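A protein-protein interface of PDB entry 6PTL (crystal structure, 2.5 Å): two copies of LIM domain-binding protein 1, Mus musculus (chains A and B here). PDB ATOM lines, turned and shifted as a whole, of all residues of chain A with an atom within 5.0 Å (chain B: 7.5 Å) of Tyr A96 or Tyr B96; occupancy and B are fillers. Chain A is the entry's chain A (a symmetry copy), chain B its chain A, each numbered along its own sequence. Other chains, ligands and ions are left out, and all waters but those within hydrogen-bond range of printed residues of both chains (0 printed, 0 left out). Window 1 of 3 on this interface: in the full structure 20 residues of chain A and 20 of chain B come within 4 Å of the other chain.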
ATOM      1  N   ASN A  31     -12.701  19.632   1.388  1.00  0.00           N
ATOM      2  CA  ASN A  31     -11.557  18.740   1.722  1.00  0.00           C
ATOM      3  C   ASN A  31     -10.634  18.604   0.505  1.00  0.00           C
ATOM      4  O   ASN A  31      -9.405  18.535   0.706  1.00  0.00           O
ATOM      5  CB  ASN A  31     -12.028  17.360   2.195  1.00  0.00           C
ATOM      6  CG  ASN A  31     -12.607  17.365   3.594  1.00  0.00           C
ATOM      7  OD1 ASN A  31     -12.378  18.292   4.368  1.00  0.00           O
ATOM      8  ND2 ASN A  31     -13.354  16.328   3.933  1.00  0.00           N
ATOM      9  N   GLU A  94      -1.624  18.776   5.971  1.00  0.00           N
ATOM     10  CA  GLU A  94      -2.968  18.350   5.494  1.00  0.00           C
ATOM     11  C   GLU A  94      -4.035  18.846   6.477  1.00  0.00           C
ATOM     12  O   GLU A  94      -3.708  19.024   7.667  1.00  0.00           O
ATOM     13  CB  GLU A  94      -3.040  16.826   5.362  1.00  0.00           C
ATOM     14  CG  GLU A  94      -1.984  16.234   4.441  1.00  0.00           C
ATOM     15  CD  GLU A  94      -2.147  16.562   2.965  1.00  0.00           C
ATOM     16  OE1 GLU A  94      -3.301  16.701   2.511  1.00  0.00           O
ATOM     17  OE2 GLU A  94      -1.117  16.673   2.273  1.00  0.00           O
ATOM     18  N   LEU A  95      -5.258  19.065   5.982  1.00  0.00           N
ATOM     19  CA  LEU A  95      -6.459  19.422   6.783  1.00  0.00           C
ATOM     20  C   LEU A  95      -7.705  18.902   6.059  1.00  0.00           C
ATOM     21  O   LEU A  95      -7.972  19.381   4.941  1.00  0.00           O
ATOM     22  CB  LEU A  95      -6.521  20.944   6.963  1.00  0.00           C
ATOM     23  CG  LEU A  95      -7.849  21.504   7.476  1.00  0.00           C
ATOM     24  CD1 LEU A  95      -8.186  20.952   8.853  1.00  0.00           C
ATOM     25  CD2 LEU A  95      -7.821  23.024   7.507  1.00  0.00           C
ATOM     26  N   TYR A  96      -8.427  17.954   6.665  1.00  0.00           N
ATOM     27  CA  TYR A  96      -9.729  17.446   6.158  1.00  0.00           C
ATOM     28  C   TYR A  96     -10.698  17.236   7.326  1.00  0.00           C
ATOM     29  O   TYR A  96     -10.245  16.945   8.452  1.00  0.00           O
ATOM     30  CB  TYR A  96      -9.543  16.174   5.324  1.00  0.00           C
ATOM     31  CG  TYR A  96      -9.005  14.973   6.060  1.00  0.00           C
ATOM     32  CD1 TYR A  96      -9.858  14.060   6.664  1.00  0.00           C
ATOM     33  CD2 TYR A  96      -7.644  14.723   6.122  1.00  0.00           C
ATOM     34  CE1 TYR A  96      -9.372  12.946   7.329  1.00  0.00           C
ATOM     35  CE2 TYR A  96      -7.141  13.613   6.782  1.00  0.00           C
ATOM     36  CZ  TYR A  96      -8.008  12.720   7.388  1.00  0.00           C
ATOM     37  OH  TYR A  96      -7.518  11.625   8.039  1.00  0.00           O
ATOM     38  N   TYR A  97     -11.993  17.396   7.044  1.00  0.00           N
ATOM     39  CA  TYR A  97     -13.122  17.235   7.996  1.00  0.00           C
ATOM     40  C   TYR A  97     -13.862  15.929   7.689  1.00  0.00           C
ATOM     41  O   TYR A  97     -14.202  15.693   6.513  1.00  0.00           O
ATOM     42  CB  TYR A  97     -14.057  18.442   7.909  1.00  0.00           C
ATOM     43  CG  TYR A  97     -13.413  19.749   8.298  1.00  0.00           C
ATOM     44  CD1 TYR A  97     -12.713  20.505   7.373  1.00  0.00           C
ATOM     45  CD2 TYR A  97     -13.491  20.223   9.598  1.00  0.00           C
ATOM     46  CE1 TYR A  97     -12.113  21.705   7.724  1.00  0.00           C
ATOM     47  CE2 TYR A  97     -12.898  21.420   9.966  1.00  0.00           C
ATOM     48  CZ  TYR A  97     -12.206  22.163   9.027  1.00  0.00           C
ATOM     49  OH  TYR A  97     -11.619  23.342   9.384  1.00  0.00           O
ATOM     50  N   VAL A  98     -14.089  15.111   8.720  1.00  0.00           N
ATOM     51  CA  VAL A  98     -14.878  13.844   8.655  1.00  0.00           C
ATOM     52  C   VAL A  98     -16.204  14.081   9.386  1.00  0.00           C
ATOM     53  O   VAL A  98     -16.157  14.454  10.574  1.00  0.00           O
ATOM     54  CB  VAL A  98     -14.102  12.660   9.262  1.00  0.00           C
ATOM     55  CG1 VAL A  98     -14.842  11.343   9.077  1.00  0.00           C
ATOM     56  CG2 VAL A  98     -12.689  12.560   8.705  1.00  0.00           C
ATOM     57  N   SER A 119     -15.153  15.480  13.051  1.00  0.00           N
ATOM     58  CA  SER A 119     -13.691  15.377  13.304  1.00  0.00           C
ATOM     59  C   SER A 119     -12.928  16.341  12.389  1.00  0.00           C
ATOM     60  O   SER A 119     -13.055  16.211  11.158  1.00  0.00           O
ATOM     61  CB  SER A 119     -13.207  13.962  13.120  1.00  0.00           C
ATOM     62  OG  SER A 119     -13.850  13.083  14.031  1.00  0.00           O
ATOM     63  N   MET A 120     -12.174  17.267  12.988  1.00  0.00           N
ATOM     64  CA  MET A 120     -11.186  18.144  12.305  1.00  0.00           C
ATOM     65  C   MET A 120      -9.803  17.493  12.430  1.00  0.00           C
ATOM     66  O   MET A 120      -9.277  17.446  13.559  1.00  0.00           O
ATOM     67  CB  MET A 120     -11.169  19.535  12.944  1.00  0.00           C
ATOM     68  CG  MET A 120     -10.088  20.448  12.410  1.00  0.00           C
ATOM     69  SD  MET A 120     -10.236  22.113  13.091  1.00  0.00           S
ATOM     70  CE  MET A 120      -8.950  22.949  12.168  1.00  0.00           C
ATOM     71  N   VAL A 121      -9.249  17.003  11.314  1.00  0.00           N
ATOM     72  CA  VAL A 121      -7.995  16.190  11.273  1.00  0.00           C
ATOM     73  C   VAL A 121      -6.907  16.985  10.543  1.00  0.00           C
ATOM     74  O   VAL A 121      -7.212  17.562   9.481  1.00  0.00           O
ATOM     75  CB  VAL A 121      -8.246  14.823  10.608  1.00  0.00           C
ATOM     76  CG1 VAL A 121      -6.996  13.954  10.607  1.00  0.00           C
ATOM     77  CG2 VAL A 121      -9.405  14.085  11.261  1.00  0.00           C
ATOM     78  N   GLN A 131      -0.219  13.612  14.183  1.00  0.00           N
ATOM     79  CA  GLN A 131      -1.588  13.873  13.659  1.00  0.00           C
ATOM     80  C   GLN A 131      -2.482  14.321  14.820  1.00  0.00           C
ATOM     81  O   GLN A 131      -2.499  13.622  15.852  1.00  0.00           O
ATOM     82  CB  GLN A 131      -2.137  12.618  12.976  1.00  0.00           C
ATOM     83  CG  GLN A 131      -3.635  12.670  12.697  1.00  0.00           C
ATOM     84  CD  GLN A 131      -4.093  11.578  11.762  1.00  0.00           C
ATOM     85  OE1 GLN A 131      -3.417  11.234  10.795  1.00  0.00           O
ATOM     86  NE2 GLN A 131      -5.262  11.025  12.042  1.00  0.00           N
ATOM     87  N   ILE B  27     -16.275   6.974  -4.017  1.00  0.00           N
ATOM     88  CA  ILE B  27     -15.395   6.617  -2.863  1.00  0.00           C
ATOM     89  C   ILE B  27     -15.859   7.392  -1.624  1.00  0.00           C
ATOM     90  O   ILE B  27     -15.721   6.848  -0.511  1.00  0.00           O
ATOM     91  CB  ILE B  27     -13.910   6.873  -3.200  1.00  0.00           C
ATOM     92  CG1 ILE B  27     -13.471   6.083  -4.436  1.00  0.00           C
ATOM     93  CG2 ILE B  27     -13.016   6.581  -2.003  1.00  0.00           C
ATOM     94  CD1 ILE B  27     -13.667   4.586  -4.321  1.00  0.00           C
ATOM     95  N   LEU B  30     -18.780   5.280  -0.677  1.00  0.00           N
ATOM     96  CA  LEU B  30     -18.231   4.019  -0.105  1.00  0.00           C
ATOM     97  C   LEU B  30     -17.807   4.264   1.347  1.00  0.00           C
ATOM     98  O   LEU B  30     -18.162   3.436   2.208  1.00  0.00           O
ATOM     99  CB  LEU B  30     -17.056   3.532  -0.959  1.00  0.00           C
ATOM    100  CG  LEU B  30     -16.451   2.191  -0.539  1.00  0.00           C
ATOM    101  CD1 LEU B  30     -16.089   1.348  -1.752  1.00  0.00           C
ATOM    102  CD2 LEU B  30     -15.233   2.389   0.352  1.00  0.00           C
ATOM    103  N   ASN B  31     -17.081   5.358   1.599  1.00  0.00           N
ATOM    104  CA  ASN B  31     -16.653   5.793   2.956  1.00  0.00           C
ATOM    105  C   ASN B  31     -17.885   6.018   3.842  1.00  0.00           C
ATOM    106  O   ASN B  31     -17.806   5.706   5.047  1.00  0.00           O
ATOM    107  CB  ASN B  31     -15.790   7.059   2.906  1.00  0.00           C
ATOM    108  CG  ASN B  31     -14.386   6.813   2.393  1.00  0.00           C
ATOM    109  OD1 ASN B  31     -13.908   5.681   2.379  1.00  0.00           O
ATOM    110  ND2 ASN B  31     -13.711   7.872   1.977  1.00  0.00           N
ATOM    111  N   LYS B  32     -18.977   6.535   3.266  1.00  0.00           N
ATOM    112  CA  LYS B  32     -20.207   6.928   4.006  1.00  0.00           C
ATOM    113  C   LYS B  32     -20.980   5.678   4.450  1.00  0.00           C
ATOM    114  O   LYS B  32     -21.514   5.698   5.574  1.00  0.00           O
ATOM    115  CB  LYS B  32     -21.097   7.842   3.158  1.00  0.00           C
ATOM    116  CG  LYS B  32     -21.825   8.919   3.949  1.00  0.00           C
ATOM    117  CD  LYS B  32     -23.068   9.448   3.271  1.00  0.00           C
ATOM    118  CE  LYS B  32     -23.564  10.736   3.892  1.00  0.00           C
ATOM    119  NZ  LYS B  32     -23.877  10.573   5.331  1.00  0.00           N
ATOM    120  N   LEU B  34     -19.671   2.759   5.069  1.00  0.00           N
ATOM    121  CA  LEU B  34     -18.794   2.111   6.085  1.00  0.00           C
ATOM    122  C   LEU B  34     -18.992   2.773   7.457  1.00  0.00           C
ATOM    123  O   LEU B  34     -18.635   2.134   8.466  1.00  0.00           O
ATOM    124  CB  LEU B  34     -17.334   2.195   5.630  1.00  0.00           C
ATOM    125  CG  LEU B  34     -16.973   1.329   4.422  1.00  0.00           C
ATOM    126  CD1 LEU B  34     -15.584   1.668   3.904  1.00  0.00           C
ATOM    127  CD2 LEU B  34     -17.070  -0.151   4.759  1.00  0.00           C
ATOM    128  N   GLN B  35     -19.532   3.997   7.494  1.00  0.00           N
ATOM    129  CA  GLN B  35     -19.889   4.725   8.744  1.00  0.00           C
ATOM    130  C   GLN B  35     -21.104   4.064   9.410  1.00  0.00           C
ATOM    131  O   GLN B  35     -21.234   4.194  10.643  1.00  0.00           O
ATOM    132  CB  GLN B  35     -20.181   6.198   8.449  1.00  0.00           C
ATOM    133  CG  GLN B  35     -18.935   7.025   8.164  1.00  0.00           C
ATOM    134  CD  GLN B  35     -19.257   8.436   7.735  1.00  0.00           C
ATOM    135  OE1 GLN B  35     -20.415   8.847   7.684  1.00  0.00           O
ATOM    136  NE2 GLN B  35     -18.222   9.198   7.421  1.00  0.00           N
ATOM    137  N   PHE B  88     -12.511  -5.223  10.169  1.00  0.00           N
ATOM    138  CA  PHE B  88     -13.255  -4.870  11.410  1.00  0.00           C
ATOM    139  C   PHE B  88     -13.092  -5.980  12.454  1.00  0.00           C
ATOM    140  O   PHE B  88     -12.887  -5.658  13.642  1.00  0.00           O
ATOM    141  CB  PHE B  88     -14.733  -4.611  11.107  1.00  0.00           C
ATOM    142  CG  PHE B  88     -14.989  -3.351  10.322  1.00  0.00           C
ATOM    143  CD1 PHE B  88     -15.317  -2.167  10.965  1.00  0.00           C
ATOM    144  CD2 PHE B  88     -14.885  -3.345   8.941  1.00  0.00           C
ATOM    145  CE1 PHE B  88     -15.547  -1.007  10.239  1.00  0.00           C
ATOM    146  CE2 PHE B  88     -15.111  -2.184   8.217  1.00  0.00           C
ATOM    147  CZ  PHE B  88     -15.444  -1.018   8.867  1.00  0.00           C
ATOM    148  N   GLU B  94     -13.654   1.994  12.616  1.00  0.00           N
ATOM    149  CA  GLU B  94     -13.857   2.870  11.430  1.00  0.00           C
ATOM    150  C   GLU B  94     -12.927   2.414  10.299  1.00  0.00           C
ATOM    151  O   GLU B  94     -11.867   1.832  10.601  1.00  0.00           O
ATOM    152  CB  GLU B  94     -13.580   4.334  11.782  1.00  0.00           C
ATOM    153  CG  GLU B  94     -14.424   4.864  12.931  1.00  0.00           C
ATOM    154  CD  GLU B  94     -15.908   5.016  12.635  1.00  0.00           C
ATOM    155  OE1 GLU B  94     -16.255   5.313  11.474  1.00  0.00           O
ATOM    156  OE2 GLU B  94     -16.712   4.839  13.571  1.00  0.00           O
ATOM    157  N   LEU B  95     -13.328   2.667   9.049  1.00  0.00           N
ATOM    158  CA  LEU B  95     -12.522   2.425   7.822  1.00  0.00           C
ATOM    159  C   LEU B  95     -12.947   3.431   6.748  1.00  0.00           C
ATOM    160  O   LEU B  95     -14.116   3.370   6.322  1.00  0.00           O
ATOM    161  CB  LEU B  95     -12.738   0.984   7.343  1.00  0.00           C
ATOM    162  CG  LEU B  95     -12.248   0.667   5.929  1.00  0.00           C
ATOM    163  CD1 LEU B  95     -10.746   0.881   5.804  1.00  0.00           C
ATOM    164  CD2 LEU B  95     -12.615  -0.753   5.532  1.00  0.00           C
ATOM    165  N   TYR B  96     -12.042   4.326   6.339  1.00  0.00           N
ATOM    166  CA  TYR B  96     -12.256   5.275   5.216  1.00  0.00           C
ATOM    167  C   TYR B  96     -10.976   5.394   4.382  1.00  0.00           C
ATOM    168  O   TYR B  96      -9.869   5.231   4.933  1.00  0.00           O
ATOM    169  CB  TYR B  96     -12.747   6.636   5.722  1.00  0.00           C
ATOM    170  CG  TYR B  96     -11.787   7.401   6.597  1.00  0.00           C
ATOM    171  CD1 TYR B  96     -10.878   8.297   6.053  1.00  0.00           C
ATOM    172  CD2 TYR B  96     -11.809   7.261   7.976  1.00  0.00           C
ATOM    173  CE1 TYR B  96     -10.003   9.016   6.853  1.00  0.00           C
ATOM    174  CE2 TYR B  96     -10.941   7.972   8.790  1.00  0.00           C
ATOM    175  CZ  TYR B  96     -10.035   8.854   8.226  1.00  0.00           C
ATOM    176  OH  TYR B  96      -9.178   9.557   9.023  1.00  0.00           O
ATOM    177  N   TYR B  97     -11.149   5.662   3.085  1.00  0.00           N
ATOM    178  CA  TYR B  97     -10.072   5.838   2.077  1.00  0.00           C
ATOM    179  C   TYR B  97      -9.948   7.323   1.722  1.00  0.00           C
ATOM    180  O   TYR B  97     -10.979   7.958   1.424  1.00  0.00           O
ATOM    181  CB  TYR B  97     -10.368   4.989   0.840  1.00  0.00           C
ATOM    182  CG  TYR B  97     -10.403   3.505   1.106  1.00  0.00           C
ATOM    183  CD1 TYR B  97     -11.563   2.883   1.537  1.00  0.00           C
ATOM    184  CD2 TYR B  97      -9.271   2.724   0.940  1.00  0.00           C
ATOM    185  CE1 TYR B  97     -11.602   1.520   1.788  1.00  0.00           C
ATOM    186  CE2 TYR B  97      -9.292   1.361   1.187  1.00  0.00           C
ATOM    187  CZ  TYR B  97     -10.461   0.756   1.613  1.00  0.00           C
ATOM    188  OH  TYR B  97     -10.487  -0.586   1.859  1.00  0.00           O
ATOM    189  N   VAL B  98      -8.722   7.851   1.766  1.00  0.00           N
ATOM    190  CA  VAL B  98      -8.370   9.245   1.360  1.00  0.00           C
ATOM    191  C   VAL B  98      -7.587   9.166   0.045  1.00  0.00           C
ATOM    192  O   VAL B  98      -6.549   8.477   0.024  1.00  0.00           O
ATOM    193  CB  VAL B  98      -7.564   9.969   2.455  1.00  0.00           C
ATOM    194  CG1 VAL B  98      -7.320  11.429   2.107  1.00  0.00           C
ATOM    195  CG2 VAL B  98      -8.224   9.850   3.821  1.00  0.00           C
ATOM    196  N   SER B 119      -4.546   6.576   0.781  1.00  0.00           N
ATOM    197  CA  SER B 119      -4.435   6.221   2.221  1.00  0.00           C
ATOM    198  C   SER B 119      -5.645   5.387   2.655  1.00  0.00           C
ATOM    199  O   SER B 119      -6.780   5.884   2.529  1.00  0.00           O
ATOM    200  CB  SER B 119      -4.296   7.455   3.075  1.00  0.00           C
ATOM    201  OG  SER B 119      -3.124   8.180   2.732  1.00  0.00           O
ATOM    202  N   MET B 120      -5.392   4.168   3.139  1.00  0.00           N
ATOM    203  CA  MET B 120      -6.382   3.292   3.820  1.00  0.00           C
ATOM    204  C   MET B 120      -6.242   3.500   5.334  1.00  0.00           C
ATOM    205  O   MET B 120      -5.202   3.091   5.888  1.00  0.00           O
ATOM    206  CB  MET B 120      -6.131   1.823   3.468  1.00  0.00           C
ATOM    207  CG  MET B 120      -6.997   0.848   4.234  1.00  0.00           C
ATOM    208  SD  MET B 120      -6.760  -0.844   3.649  1.00  0.00           S
ATOM    209  CE  MET B 120      -8.002  -1.692   4.620  1.00  0.00           C
ATOM    210  N   VAL B 121      -7.245   4.120   5.965  1.00  0.00           N
ATOM    211  CA  VAL B 121      -7.209   4.558   7.394  1.00  0.00           C
ATOM    212  C   VAL B 121      -8.233   3.744   8.193  1.00  0.00           C
ATOM    213  O   VAL B 121      -9.368   3.586   7.706  1.00  0.00           O
ATOM    214  CB  VAL B 121      -7.465   6.073   7.515  1.00  0.00           C
ATOM    215  CG1 VAL B 121      -7.375   6.551   8.957  1.00  0.00           C
ATOM    216  CG2 VAL B 121      -6.522   6.873   6.629  1.00  0.00           C
ATOM    217  N   THR B 122      -7.836   3.262   9.378  1.00  0.00           N
ATOM    218  CA  THR B 122      -8.663   2.442  10.306  1.00  0.00           C
ATOM    219  C   THR B 122      -8.427   2.893  11.754  1.00  0.00           C
ATOM    220  O   THR B 122      -7.249   3.003  12.147  1.00  0.00           O
ATOM    221  CB  THR B 122      -8.349   0.947  10.161  1.00  0.00           C
ATOM    222  OG1 THR B 122      -6.931   0.791  10.124  1.00  0.00           O
ATOM    223  CG2 THR B 122      -8.958   0.329   8.923  1.00  0.00           C
ATOM    224  N   GLN B 123      -9.507   3.137  12.506  1.00  0.00           N
ATOM    225  CA  GLN B 123      -9.490   3.396  13.974  1.00  0.00           C
ATOM    226  C   GLN B 123      -9.785   2.080  14.704  1.00  0.00           C
ATOM    227  O   GLN B 123     -10.783   1.425  14.343  1.00  0.00           O
ATOM    228  CB  GLN B 123     -10.518   4.465  14.356  1.00  0.00           C
ATOM    229  CG  GLN B 123     -10.050   5.891  14.102  1.00  0.00           C
ATOM    230  CD  GLN B 123     -11.048   6.922  14.571  1.00  0.00           C
ATOM    231  OE1 GLN B 123     -11.800   6.706  15.519  1.00  0.00           O
ATOM    232  NE2 GLN B 123     -11.057   8.066  13.907  1.00  0.00           N
ATOM    233  N   GLN B 131      -4.584   4.110  15.671  1.00  0.00           N
ATOM    234  CA  GLN B 131      -5.007   4.370  14.268  1.00  0.00           C
ATOM    235  C   GLN B 131      -3.913   3.863  13.321  1.00  0.00           C
ATOM    236  O   GLN B 131      -2.740   4.227  13.534  1.00  0.00           O
ATOM    237  CB  GLN B 131      -5.278   5.864  14.069  1.00  0.00           C
ATOM    238  CG  GLN B 131      -5.398   6.282  12.608  1.00  0.00           C
ATOM    239  CD  GLN B 131      -5.962   7.671  12.443  1.00  0.00           C
ATOM    240  OE1 GLN B 131      -6.874   8.084  13.157  1.00  0.00           O
ATOM    241  NE2 GLN B 131      -5.423   8.408  11.485  1.00  0.00           N
ATOM    242  N   VAL B 132      -4.292   3.058  12.322  1.00  0.00           N
ATOM    243  CA  VAL B 132      -3.375   2.500  11.283  1.00  0.00           C
ATOM    244  C   VAL B 132      -3.655   3.219   9.959  1.00  0.00           C
ATOM    245  O   VAL B 132      -4.835   3.282   9.561  1.00  0.00           O
ATOM    246  CB  VAL B 132      -3.532   0.974  11.141  1.00  0.00           C
ATOM    247  CG1 VAL B 132      -2.478   0.379  10.218  1.00  0.00           C
ATOM    248  CG2 VAL B 132      -3.506   0.275  12.491  1.00  0.00           C
ATOM    249  N   CYS B 133      -2.604   3.735   9.315  1.00  0.00           N
ATOM    250  CA  CYS B 133      -2.656   4.513   8.047  1.00  0.00           C
ATOM    251  C   CYS B 133      -1.766   3.838   6.996  1.00  0.00           C
ATOM    252  O   CYS B 133      -0.571   4.187   6.917  1.00  0.00           O
ATOM    253  CB  CYS B 133      -2.217   5.955   8.283  1.00  0.00           C
ATOM    254  SG  CYS B 133      -2.010   6.910   6.756  1.00  0.00           S
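O of Tyr A96 is in hydrogen-bond range of N of Val A121 (3.0 Å). N of Val B121 is in hydrogen-bond range of O of Tyr B96 (3.0 Å).
The side-chain hydroxyl (OH) of Tyr B96 lies within hydrogen-bond range of the side-chain hydroxyl (OH) of Tyr A96, at 2.8 Å. The side-chain amide nitrogen (NE2) of Gln B131 sits close to the side-chain amide nitrogen (NE2) of Gln A131 (2.7 Å).
Tyr B96 touches its own counterpart, Tyr A96. Gln A131 touches its own counterpart, Gln B131. 10 positions are printed for both chains.
Tyr A96 touches just one residue of chain B: Tyr B96 (2.8 Å). Of the printed residues of chain B, Gln A131 touches Gln B131 (2.7 Å). Tyr B96 touches one residue of chain A. Printed residues of chain A within 4 Å of Gln B131: Gln A131 (2.7 Å).
Hydrophobic or aromatic side chains of chain B within 4 Å of the printed part of chain A: Tyr B96. Of the 10 printed residues of chain A, 2 touch a printed residue of chain B. Hydrophobic or aromatic side chains of chain A that line the printed part of chain B: Tyr A96. Among the printed residues, no Asp or Glu carboxylate lies within 4 Å of a Lys or Arg side-chain nitrogen of the other chain.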
